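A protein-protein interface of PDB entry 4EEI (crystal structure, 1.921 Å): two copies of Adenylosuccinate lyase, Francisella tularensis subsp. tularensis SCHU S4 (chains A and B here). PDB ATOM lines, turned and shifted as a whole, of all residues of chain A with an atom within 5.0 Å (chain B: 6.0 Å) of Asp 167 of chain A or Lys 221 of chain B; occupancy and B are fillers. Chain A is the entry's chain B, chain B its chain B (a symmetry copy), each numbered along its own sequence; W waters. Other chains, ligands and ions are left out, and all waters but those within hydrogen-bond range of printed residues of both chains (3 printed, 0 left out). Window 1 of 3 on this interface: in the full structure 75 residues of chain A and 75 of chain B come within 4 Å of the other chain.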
ATOM      1  N   ARG A 163     -33.646 -25.390  -3.698  1.00  0.00           N
ATOM      2  CA  ARG A 163     -33.297 -26.251  -4.827  1.00  0.00           C
ATOM      3  C   ARG A 163     -32.267 -27.280  -4.360  1.00  0.00           C
ATOM      4  O   ARG A 163     -32.340 -28.454  -4.732  1.00  0.00           O
ATOM      5  CB  ARG A 163     -32.767 -25.433  -6.015  1.00  0.00           C
ATOM      6  CG  ARG A 163     -33.846 -24.644  -6.755  1.00  0.00           C
ATOM      7  CD  ARG A 163     -33.325 -24.043  -8.076  1.00  0.00           C
ATOM      8  NE  ARG A 163     -32.368 -22.939  -7.904  1.00  0.00           N
ATOM      9  CZ  ARG A 163     -32.723 -21.670  -7.722  1.00  0.00           C
ATOM     10  NH1 ARG A 163     -34.009 -21.342  -7.635  1.00  0.00           N
ATOM     11  NH2 ARG A 163     -31.802 -20.723  -7.615  1.00  0.00           N
ATOM     12  N   ARG A 164     -31.324 -26.846  -3.528  1.00  0.00           N
ATOM     13  CA  ARG A 164     -30.304 -27.763  -3.011  1.00  0.00           C
ATOM     14  C   ARG A 164     -30.913 -28.745  -2.015  1.00  0.00           C
ATOM     15  O   ARG A 164     -30.529 -29.919  -1.974  1.00  0.00           O
ATOM     16  CB  ARG A 164     -29.161 -26.988  -2.357  1.00  0.00           C
ATOM     17  CG  ARG A 164     -28.472 -25.982  -3.279  1.00  0.00           C
ATOM     18  CD  ARG A 164     -27.578 -26.653  -4.342  1.00  0.00           C
ATOM     19  NE  ARG A 164     -28.354 -27.239  -5.440  1.00  0.00           N
ATOM     20  CZ  ARG A 164     -28.867 -26.541  -6.452  1.00  0.00           C
ATOM     21  NH1 ARG A 164     -29.573 -27.151  -7.394  1.00  0.00           N
ATOM     22  NH2 ARG A 164     -28.668 -25.229  -6.521  1.00  0.00           N
ATOM     23  N   LEU A 165     -31.871 -28.274  -1.221  1.00  0.00           N
ATOM     24  CA  LEU A 165     -32.514 -29.151  -0.246  1.00  0.00           C
ATOM     25  C   LEU A 165     -33.260 -30.274  -0.956  1.00  0.00           C
ATOM     26  O   LEU A 165     -33.216 -31.430  -0.529  1.00  0.00           O
ATOM     27  CB  LEU A 165     -33.442 -28.357   0.696  1.00  0.00           C
ATOM     28  CG  LEU A 165     -34.194 -29.199   1.731  1.00  0.00           C
ATOM     29  CD1 LEU A 165     -33.217 -29.835   2.721  1.00  0.00           C
ATOM     30  CD2 LEU A 165     -35.216 -28.347   2.467  1.00  0.00           C
ATOM     31  N   LYS A 166     -33.938 -29.954  -2.055  1.00  0.00           N
ATOM     32  CA  LYS A 166     -34.593 -31.005  -2.821  1.00  0.00           C
ATOM     33  C   LYS A 166     -33.579 -32.002  -3.400  1.00  0.00           C
ATOM     34  O   LYS A 166     -33.824 -33.205  -3.373  1.00  0.00           O
ATOM     35  CB  LYS A 166     -35.487 -30.432  -3.928  1.00  0.00           C
ATOM     36  CG  LYS A 166     -36.258 -31.511  -4.694  1.00  0.00           C
ATOM     37  CD  LYS A 166     -37.014 -30.923  -5.875  1.00  0.00           C
ATOM     38  CE  LYS A 166     -37.680 -32.015  -6.724  1.00  0.00           C
ATOM     39  NZ  LYS A 166     -36.708 -32.866  -7.492  1.00  0.00           N
ATOM     40  N   ASP A 167     -32.454 -31.510  -3.921  1.00  0.00           N
ATOM     41  CA  ASP A 167     -31.395 -32.401  -4.424  1.00  0.00           C
ATOM     42  C   ASP A 167     -30.964 -33.380  -3.327  1.00  0.00           C
ATOM     43  O   ASP A 167     -30.803 -34.575  -3.583  1.00  0.00           O
ATOM     44  CB  ASP A 167     -30.150 -31.609  -4.866  1.00  0.00           C
ATOM     45  CG  ASP A 167     -30.381 -30.754  -6.109  1.00  0.00           C
ATOM     46  OD1 ASP A 167     -31.360 -31.012  -6.843  1.00  0.00           O
ATOM     47  OD2 ASP A 167     -29.553 -29.829  -6.358  1.00  0.00           O
ATOM     48  N   LEU A 168     -30.760 -32.872  -2.114  1.00  0.00           N
ATOM     49  CA  LEU A 168     -30.278 -33.710  -1.010  1.00  0.00           C
ATOM     50  C   LEU A 168     -31.327 -34.722  -0.553  1.00  0.00           C
ATOM     51  O   LEU A 168     -31.008 -35.889  -0.276  1.00  0.00           O
ATOM     52  CB  LEU A 168     -29.820 -32.862   0.184  1.00  0.00           C
ATOM     53  CG  LEU A 168     -28.451 -32.200   0.132  1.00  0.00           C
ATOM     54  CD1 LEU A 168     -28.128 -31.561   1.469  1.00  0.00           C
ATOM     55  CD2 LEU A 168     -27.380 -33.212  -0.240  1.00  0.00           C
ATOM     56  N   LYS A 169     -32.578 -34.280  -0.466  1.00  0.00           N
ATOM     57  CA  LYS A 169     -33.648 -35.183  -0.069  1.00  0.00           C
ATOM     58  C   LYS A 169     -33.854 -36.261  -1.144  1.00  0.00           C
ATOM     59  O   LYS A 169     -34.182 -37.409  -0.827  1.00  0.00           O
ATOM     60  CB  LYS A 169     -34.938 -34.407   0.217  1.00  0.00           C
ATOM     61  CG  LYS A 169     -34.896 -33.616   1.539  1.00  0.00           C
ATOM     62  CD  LYS A 169     -36.234 -32.939   1.826  1.00  0.00           C
ATOM     63  CE  LYS A 169     -36.292 -32.419   3.257  1.00  0.00           C
ATOM     64  NZ  LYS A 169     -37.527 -31.638   3.556  1.00  0.00           N
ATOM     65  N   ASP A 170     -33.655 -35.898  -2.408  1.00  0.00           N
ATOM     66  CA  ASP A 170     -33.706 -36.884  -3.487  1.00  0.00           C
ATOM     67  C   ASP A 170     -32.602 -37.920  -3.314  1.00  0.00           C
ATOM     68  O   ASP A 170     -32.823 -39.118  -3.489  1.00  0.00           O
ATOM     69  CB  ASP A 170     -33.564 -36.223  -4.862  1.00  0.00           C
ATOM     70  CG  ASP A 170     -34.837 -35.519  -5.314  1.00  0.00           C
ATOM     71  OD1 ASP A 170     -35.913 -35.807  -4.747  1.00  0.00           O
ATOM     72  OD2 ASP A 170     -34.753 -34.683  -6.246  1.00  0.00           O
ATOM     73  N   PHE A 171     -31.406 -37.457  -2.985  1.00  0.00           N
ATOM     74  CA  PHE A 171     -30.278 -38.371  -2.810  1.00  0.00           C
ATOM     75  C   PHE A 171     -30.524 -39.231  -1.588  1.00  0.00           C
ATOM     76  O   PHE A 171     -30.189 -40.410  -1.570  1.00  0.00           O
ATOM     77  CB  PHE A 171     -28.981 -37.602  -2.629  1.00  0.00           C
ATOM     78  CG  PHE A 171     -27.755 -38.472  -2.672  1.00  0.00           C
ATOM     79  CD1 PHE A 171     -27.224 -39.014  -1.509  1.00  0.00           C
ATOM     80  CD2 PHE A 171     -27.136 -38.747  -3.875  1.00  0.00           C
ATOM     81  CE1 PHE A 171     -26.077 -39.826  -1.558  1.00  0.00           C
ATOM     82  CE2 PHE A 171     -25.995 -39.558  -3.936  1.00  0.00           C
ATOM     83  CZ  PHE A 171     -25.469 -40.099  -2.778  1.00  0.00           C
ATOM     84  N   ILE A 225     -23.303 -32.079  -5.115  1.00  0.00           N
ATOM     85  CA  ILE A 225     -24.396 -31.297  -4.535  1.00  0.00           C
ATOM     86  C   ILE A 225     -23.856 -30.354  -3.451  1.00  0.00           C
ATOM     87  O   ILE A 225     -24.266 -29.193  -3.347  1.00  0.00           O
ATOM     88  CB  ILE A 225     -25.488 -32.196  -3.933  1.00  0.00           C
ATOM     89  CG1 ILE A 225     -26.127 -33.062  -5.020  1.00  0.00           C
ATOM     90  CG2 ILE A 225     -26.564 -31.350  -3.239  1.00  0.00           C
ATOM     91  CD1 ILE A 225     -27.024 -34.164  -4.456  1.00  0.00           C
ATOM     92  N   LEU A 228     -22.419 -27.299  -4.960  1.00  0.00           N
ATOM     93  CA  LEU A 228     -23.435 -26.331  -5.383  1.00  0.00           C
ATOM     94  C   LEU A 228     -23.950 -25.549  -4.184  1.00  0.00           C
ATOM     95  O   LEU A 228     -24.221 -24.340  -4.283  1.00  0.00           O
ATOM     96  CB  LEU A 228     -24.598 -27.044  -6.076  1.00  0.00           C
ATOM     97  CG  LEU A 228     -24.301 -27.701  -7.425  1.00  0.00           C
ATOM     98  CD1 LEU A 228     -25.445 -28.618  -7.813  1.00  0.00           C
ATOM     99  CD2 LEU A 228     -24.119 -26.644  -8.505  1.00  0.00           C
ATOM    100  N   PHE B 171     -33.231 -33.388 -15.035  1.00  0.00           N
ATOM    101  CA  PHE B 171     -32.950 -31.970 -15.253  1.00  0.00           C
ATOM    102  C   PHE B 171     -33.752 -31.485 -16.444  1.00  0.00           C
ATOM    103  O   PHE B 171     -34.242 -30.362 -16.457  1.00  0.00           O
ATOM    104  CB  PHE B 171     -31.473 -31.744 -15.519  1.00  0.00           C
ATOM    105  CG  PHE B 171     -31.077 -30.293 -15.526  1.00  0.00           C
ATOM    106  CD1 PHE B 171     -31.074 -29.560 -16.705  1.00  0.00           C
ATOM    107  CD2 PHE B 171     -30.709 -29.665 -14.353  1.00  0.00           C
ATOM    108  CE1 PHE B 171     -30.702 -28.204 -16.702  1.00  0.00           C
ATOM    109  CE2 PHE B 171     -30.340 -28.314 -14.338  1.00  0.00           C
ATOM    110  CZ  PHE B 171     -30.340 -27.584 -15.511  1.00  0.00           C
ATOM    111  N   ASP B 174     -37.093 -30.641 -15.281  1.00  0.00           N
ATOM    112  CA  ASP B 174     -37.080 -29.563 -14.289  1.00  0.00           C
ATOM    113  C   ASP B 174     -35.651 -29.053 -14.048  1.00  0.00           C
ATOM    114  O   ASP B 174     -34.939 -29.567 -13.173  1.00  0.00           O
ATOM    115  CB  ASP B 174     -37.686 -30.084 -12.981  1.00  0.00           C
ATOM    116  CG  ASP B 174     -37.637 -29.067 -11.845  1.00  0.00           C
ATOM    117  OD1 ASP B 174     -37.429 -27.860 -12.101  1.00  0.00           O
ATOM    118  OD2 ASP B 174     -37.828 -29.485 -10.681  1.00  0.00           O
ATOM    119  N   ARG B 216     -27.237 -18.559 -11.671  1.00  0.00           N
ATOM    120  CA  ARG B 216     -26.326 -19.426 -12.414  1.00  0.00           C
ATOM    121  C   ARG B 216     -26.175 -20.828 -11.852  1.00  0.00           C
ATOM    122  O   ARG B 216     -25.455 -21.647 -12.436  1.00  0.00           O
ATOM    123  CB  ARG B 216     -24.955 -18.752 -12.572  1.00  0.00           C
ATOM    124  CG  ARG B 216     -24.649 -18.324 -14.012  1.00  0.00           C
ATOM    125  CD  ARG B 216     -25.740 -17.408 -14.569  1.00  0.00           C
ATOM    126  NE  ARG B 216     -25.603 -17.191 -16.015  1.00  0.00           N
ATOM    127  CZ  ARG B 216     -26.499 -16.551 -16.760  1.00  0.00           C
ATOM    128  NH1 ARG B 216     -27.601 -16.066 -16.201  1.00  0.00           N
ATOM    129  NH2 ARG B 216     -26.295 -16.390 -18.057  1.00  0.00           N
ATOM    130  N   ASP B 217     -26.859 -21.129 -10.748  1.00  0.00           N
ATOM    131  CA  ASP B 217     -26.760 -22.470 -10.160  1.00  0.00           C
ATOM    132  C   ASP B 217     -27.493 -23.534 -10.977  1.00  0.00           C
ATOM    133  O   ASP B 217     -27.251 -24.740 -10.809  1.00  0.00           O
ATOM    134  CB  ASP B 217     -27.235 -22.490  -8.698  1.00  0.00           C
ATOM    135  CG  ASP B 217     -28.736 -22.238  -8.561  1.00  0.00           C
ATOM    136  OD1 ASP B 217     -29.505 -23.210  -8.356  1.00  0.00           O
ATOM    137  OD2 ASP B 217     -29.137 -21.060  -8.646  1.00  0.00           O
ATOM    138  N   ARG B 218     -28.393 -23.102 -11.856  1.00  0.00           N
ATOM    139  CA  ARG B 218     -29.070 -24.053 -12.736  1.00  0.00           C
ATOM    140  C   ARG B 218     -28.065 -24.559 -13.749  1.00  0.00           C
ATOM    141  O   ARG B 218     -27.918 -25.766 -13.947  1.00  0.00           O
ATOM    142  CB  ARG B 218     -30.269 -23.400 -13.435  1.00  0.00           C
ATOM    143  CG  ARG B 218     -31.301 -22.833 -12.457  1.00  0.00           C
ATOM    144  CD  ARG B 218     -32.619 -22.494 -13.149  1.00  0.00           C
ATOM    145  NE  ARG B 218     -33.659 -22.120 -12.177  1.00  0.00           N
ATOM    146  CZ  ARG B 218     -34.496 -22.985 -11.611  1.00  0.00           C
ATOM    147  NH1 ARG B 218     -34.423 -24.277 -11.912  1.00  0.00           N
ATOM    148  NH2 ARG B 218     -35.416 -22.559 -10.756  1.00  0.00           N
ATOM    149  N   ILE B 219     -27.352 -23.633 -14.381  1.00  0.00           N
ATOM    150  CA  ILE B 219     -26.281 -24.023 -15.290  1.00  0.00           C
ATOM    151  C   ILE B 219     -25.233 -24.849 -14.556  1.00  0.00           C
ATOM    152  O   ILE B 219     -24.763 -25.859 -15.076  1.00  0.00           O
ATOM    153  CB  ILE B 219     -25.615 -22.802 -15.952  1.00  0.00           C
ATOM    154  CG1 ILE B 219     -26.538 -22.237 -17.037  1.00  0.00           C
ATOM    155  CG2 ILE B 219     -24.273 -23.198 -16.593  1.00  0.00           C
ATOM    156  CD1 ILE B 219     -26.114 -20.871 -17.572  1.00  0.00           C
ATOM    157  N   ALA B 220     -24.872 -24.431 -13.349  1.00  0.00           N
ATOM    158  CA  ALA B 220     -23.837 -25.138 -12.603  1.00  0.00           C
ATOM    159  C   ALA B 220     -24.276 -26.560 -12.273  1.00  0.00           C
ATOM    160  O   ALA B 220     -23.455 -27.477 -12.234  1.00  0.00           O
ATOM    161  CB  ALA B 220     -23.467 -24.381 -11.333  1.00  0.00           C
ATOM    162  N   LYS B 221     -25.566 -26.749 -12.018  1.00  0.00           N
ATOM    163  CA  LYS B 221     -26.055 -28.079 -11.699  1.00  0.00           C
ATOM    164  C   LYS B 221     -25.878 -29.005 -12.900  1.00  0.00           C
ATOM    165  O   LYS B 221     -25.400 -30.135 -12.755  1.00  0.00           O
ATOM    166  CB  LYS B 221     -27.527 -28.039 -11.278  1.00  0.00           C
ATOM    167  CG  LYS B 221     -28.141 -29.442 -11.144  1.00  0.00           C
ATOM    168  CD  LYS B 221     -29.507 -29.410 -10.457  1.00  0.00           C
ATOM    169  CE  LYS B 221     -30.101 -30.814 -10.354  1.00  0.00           C
ATOM    170  NZ  LYS B 221     -31.419 -30.775  -9.649  1.00  0.00           N
ATOM    171  N   LEU B 222     -26.246 -28.522 -14.087  1.00  0.00           N
ATOM    172  CA  LEU B 222     -26.115 -29.306 -15.311  1.00  0.00           C
ATOM    173  C   LEU B 222     -24.654 -29.626 -15.605  1.00  0.00           C
ATOM    174  O   LEU B 222     -24.315 -30.768 -15.933  1.00  0.00           O
ATOM    175  CB  LEU B 222     -26.734 -28.561 -16.502  1.00  0.00           C
ATOM    176  CG  LEU B 222     -26.549 -29.222 -17.876  1.00  0.00           C
ATOM    177  CD1 LEU B 222     -27.139 -30.625 -17.900  1.00  0.00           C
ATOM    178  CD2 LEU B 222     -27.176 -28.380 -18.983  1.00  0.00           C
ATOM    179  N   ILE B 223     -23.796 -28.617 -15.495  1.00  0.00           N
ATOM    180  CA  ILE B 223     -22.365 -28.812 -15.718  1.00  0.00           C
ATOM    181  C   ILE B 223     -21.774 -29.806 -14.710  1.00  0.00           C
ATOM    182  O   ILE B 223     -20.873 -30.578 -15.052  1.00  0.00           O
ATOM    183  CB  ILE B 223     -21.624 -27.455 -15.696  1.00  0.00           C
ATOM    184  CG1 ILE B 223     -22.196 -26.542 -16.783  1.00  0.00           C
ATOM    185  CG2 ILE B 223     -20.118 -27.635 -15.878  1.00  0.00           C
ATOM    186  CD1 ILE B 223     -22.017 -27.069 -18.193  1.00  0.00           C
ATOM    187  N   SER B 224     -22.287 -29.798 -13.478  1.00  0.00           N
ATOM    188  CA  SER B 224     -21.883 -30.790 -12.476  1.00  0.00           C
ATOM    189  C   SER B 224     -22.271 -32.207 -12.873  1.00  0.00           C
ATOM    190  O   SER B 224     -21.508 -33.160 -12.646  1.00  0.00           O
ATOM    191  CB  SER B 224     -22.481 -30.456 -11.108  1.00  0.00           C
ATOM    192  OG  SER B 224     -21.929 -29.239 -10.633  1.00  0.00           O
ATOM    193  N   ILE B 225     -23.456 -32.363 -13.451  1.00  0.00           N
ATOM    194  CA  ILE B 225     -23.834 -33.672 -13.986  1.00  0.00           C
ATOM    195  C   ILE B 225     -22.878 -34.079 -15.116  1.00  0.00           C
ATOM    196  O   ILE B 225     -22.463 -35.238 -15.220  1.00  0.00           O
ATOM    197  CB  ILE B 225     -25.279 -33.681 -14.511  1.00  0.00           C
ATOM    198  CG1 ILE B 225     -26.262 -33.397 -13.374  1.00  0.00           C
ATOM    199  CG2 ILE B 225     -25.609 -35.031 -15.161  1.00  0.00           C
ATOM    200  CD1 ILE B 225     -27.684 -33.125 -13.867  1.00  0.00           C
ATOM    201  N   HIS B 226     -22.530 -33.129 -15.975  1.00  0.00           N
ATOM    202  CA  HIS B 226     -21.615 -33.426 -17.074  1.00  0.00           C
ATOM    203  C   HIS B 226     -20.238 -33.826 -16.524  1.00  0.00           C
ATOM    204  O   HIS B 226     -19.545 -34.662 -17.114  1.00  0.00           O
ATOM    205  CB  HIS B 226     -21.513 -32.220 -18.016  1.00  0.00           C
ATOM    206  CG  HIS B 226     -22.677 -32.091 -18.948  1.00  0.00           C
ATOM    207  ND1 HIS B 226     -22.685 -31.213 -20.010  1.00  0.00           N
ATOM    208  CD2 HIS B 226     -23.863 -32.744 -18.989  1.00  0.00           C
ATOM    209  CE1 HIS B 226     -23.827 -31.333 -20.669  1.00  0.00           C
ATOM    210  NE2 HIS B 226     -24.558 -32.260 -20.075  1.00  0.00           N
HETATM  211  O   HOH W   1     -36.530 -22.784  -7.662  1.00  0.00           O
HETATM  212  O   HOH W   2     -34.249 -31.295  -8.269  1.00  0.00           O
HETATM  213  O   HOH W   3     -30.138 -25.533  -9.691  1.00  0.00           O
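The guanidinium group of Arg 164 of chain A lies within salt-bridge range of the side-chain carboxylate of Asp 217 of chain B (2.9 Å).
OD2 of Asp 217 of chain B is in salt-bridge range of NH2 of Arg 163 of chain A (2.9 Å).
NZ of Lys 221 of chain B lies within salt-bridge range of OD1 of Asp 167 of chain A (2.8 Å).
The guanidinium group (NH1) of Arg 164 of chain A lies within salt-bridge range of the side-chain carboxylate (OD2) of Asp 167 of chain A (2.9 Å).
The backbone carbonyl oxygen (O) of Ala 220 of chain B is in hydrogen-bond range of the side-chain hydroxyl (OG) of Ser 224 of chain B.
Water W3 lies within hydrogen-bond range of OD1 of Asp 217 of chain B and NH1 of Arg 164 of chain A.
Water W1 bridges NH1 of Arg 163 of chain A and NH2 of Arg 218 of chain B.
Water W2 lies within hydrogen-bond range of NZ of Lys 166 of chain A (3.0 Å), NZ of Lys 221 of chain B (3.2 Å) and OD1 of Asp 167 of chain A (3.2 Å).
Positions printed for both chains: 171 and 225.
Of the 13 printed residues of chain B, 4 touch a printed residue of chain A.
Of the 11 printed residues of chain A, 4 touch a printed residue of chain B.
Among the printed residues, Asp or Glu carboxylates within 4 Å of a Lys or Arg side-chain nitrogen of the other chain: Arg 163 of chain A with Asp 217 of chain B (2.9 Å), Arg 164 of chain A with Asp 217 of chain B (2.9 Å) and Asp 167 of chain A with Lys 221 of chain B (2.8 Å).
Of the printed residues of chain B, Arg 163 of chain A touches Asp 217 and Arg 218.
Printed residues of chain B within 4 Å of Arg 164 of chain A: Asp 217 and Lys 221.
Asp 167 of chain A touches one residue of chain B.
Printed residues of chain A within 4 Å of Ala 220 of chain B: Leu 228 (3.7 Å).
Of the printed residues of chain A, Lys 221 of chain B touches Arg 164 (3.8 Å), Asp 167 (2.8 Å) and Leu 228 (3.8 Å).
The nearest printed residue of chain A that does not touch Lys 221 of chain B is Arg 163 of chain A (5.5 Å).
The nearest printed residue of chain A that does not touch Ala 220 of chain B is Arg 164 of chain A (7.1 Å).
Arg 163 of chain A touches Arg 218 of chain B.
CD of Lys 221 of chain B touches NH1 of Arg 164 of chain A, 3.8 Å away.
CD2 of Leu 228 of chain A touches CB of Ala 220 of chain B, at 3.7 Å.
CD2 of Leu 228 of chain A touches N of Lys 221 of chain B (3.8 Å).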
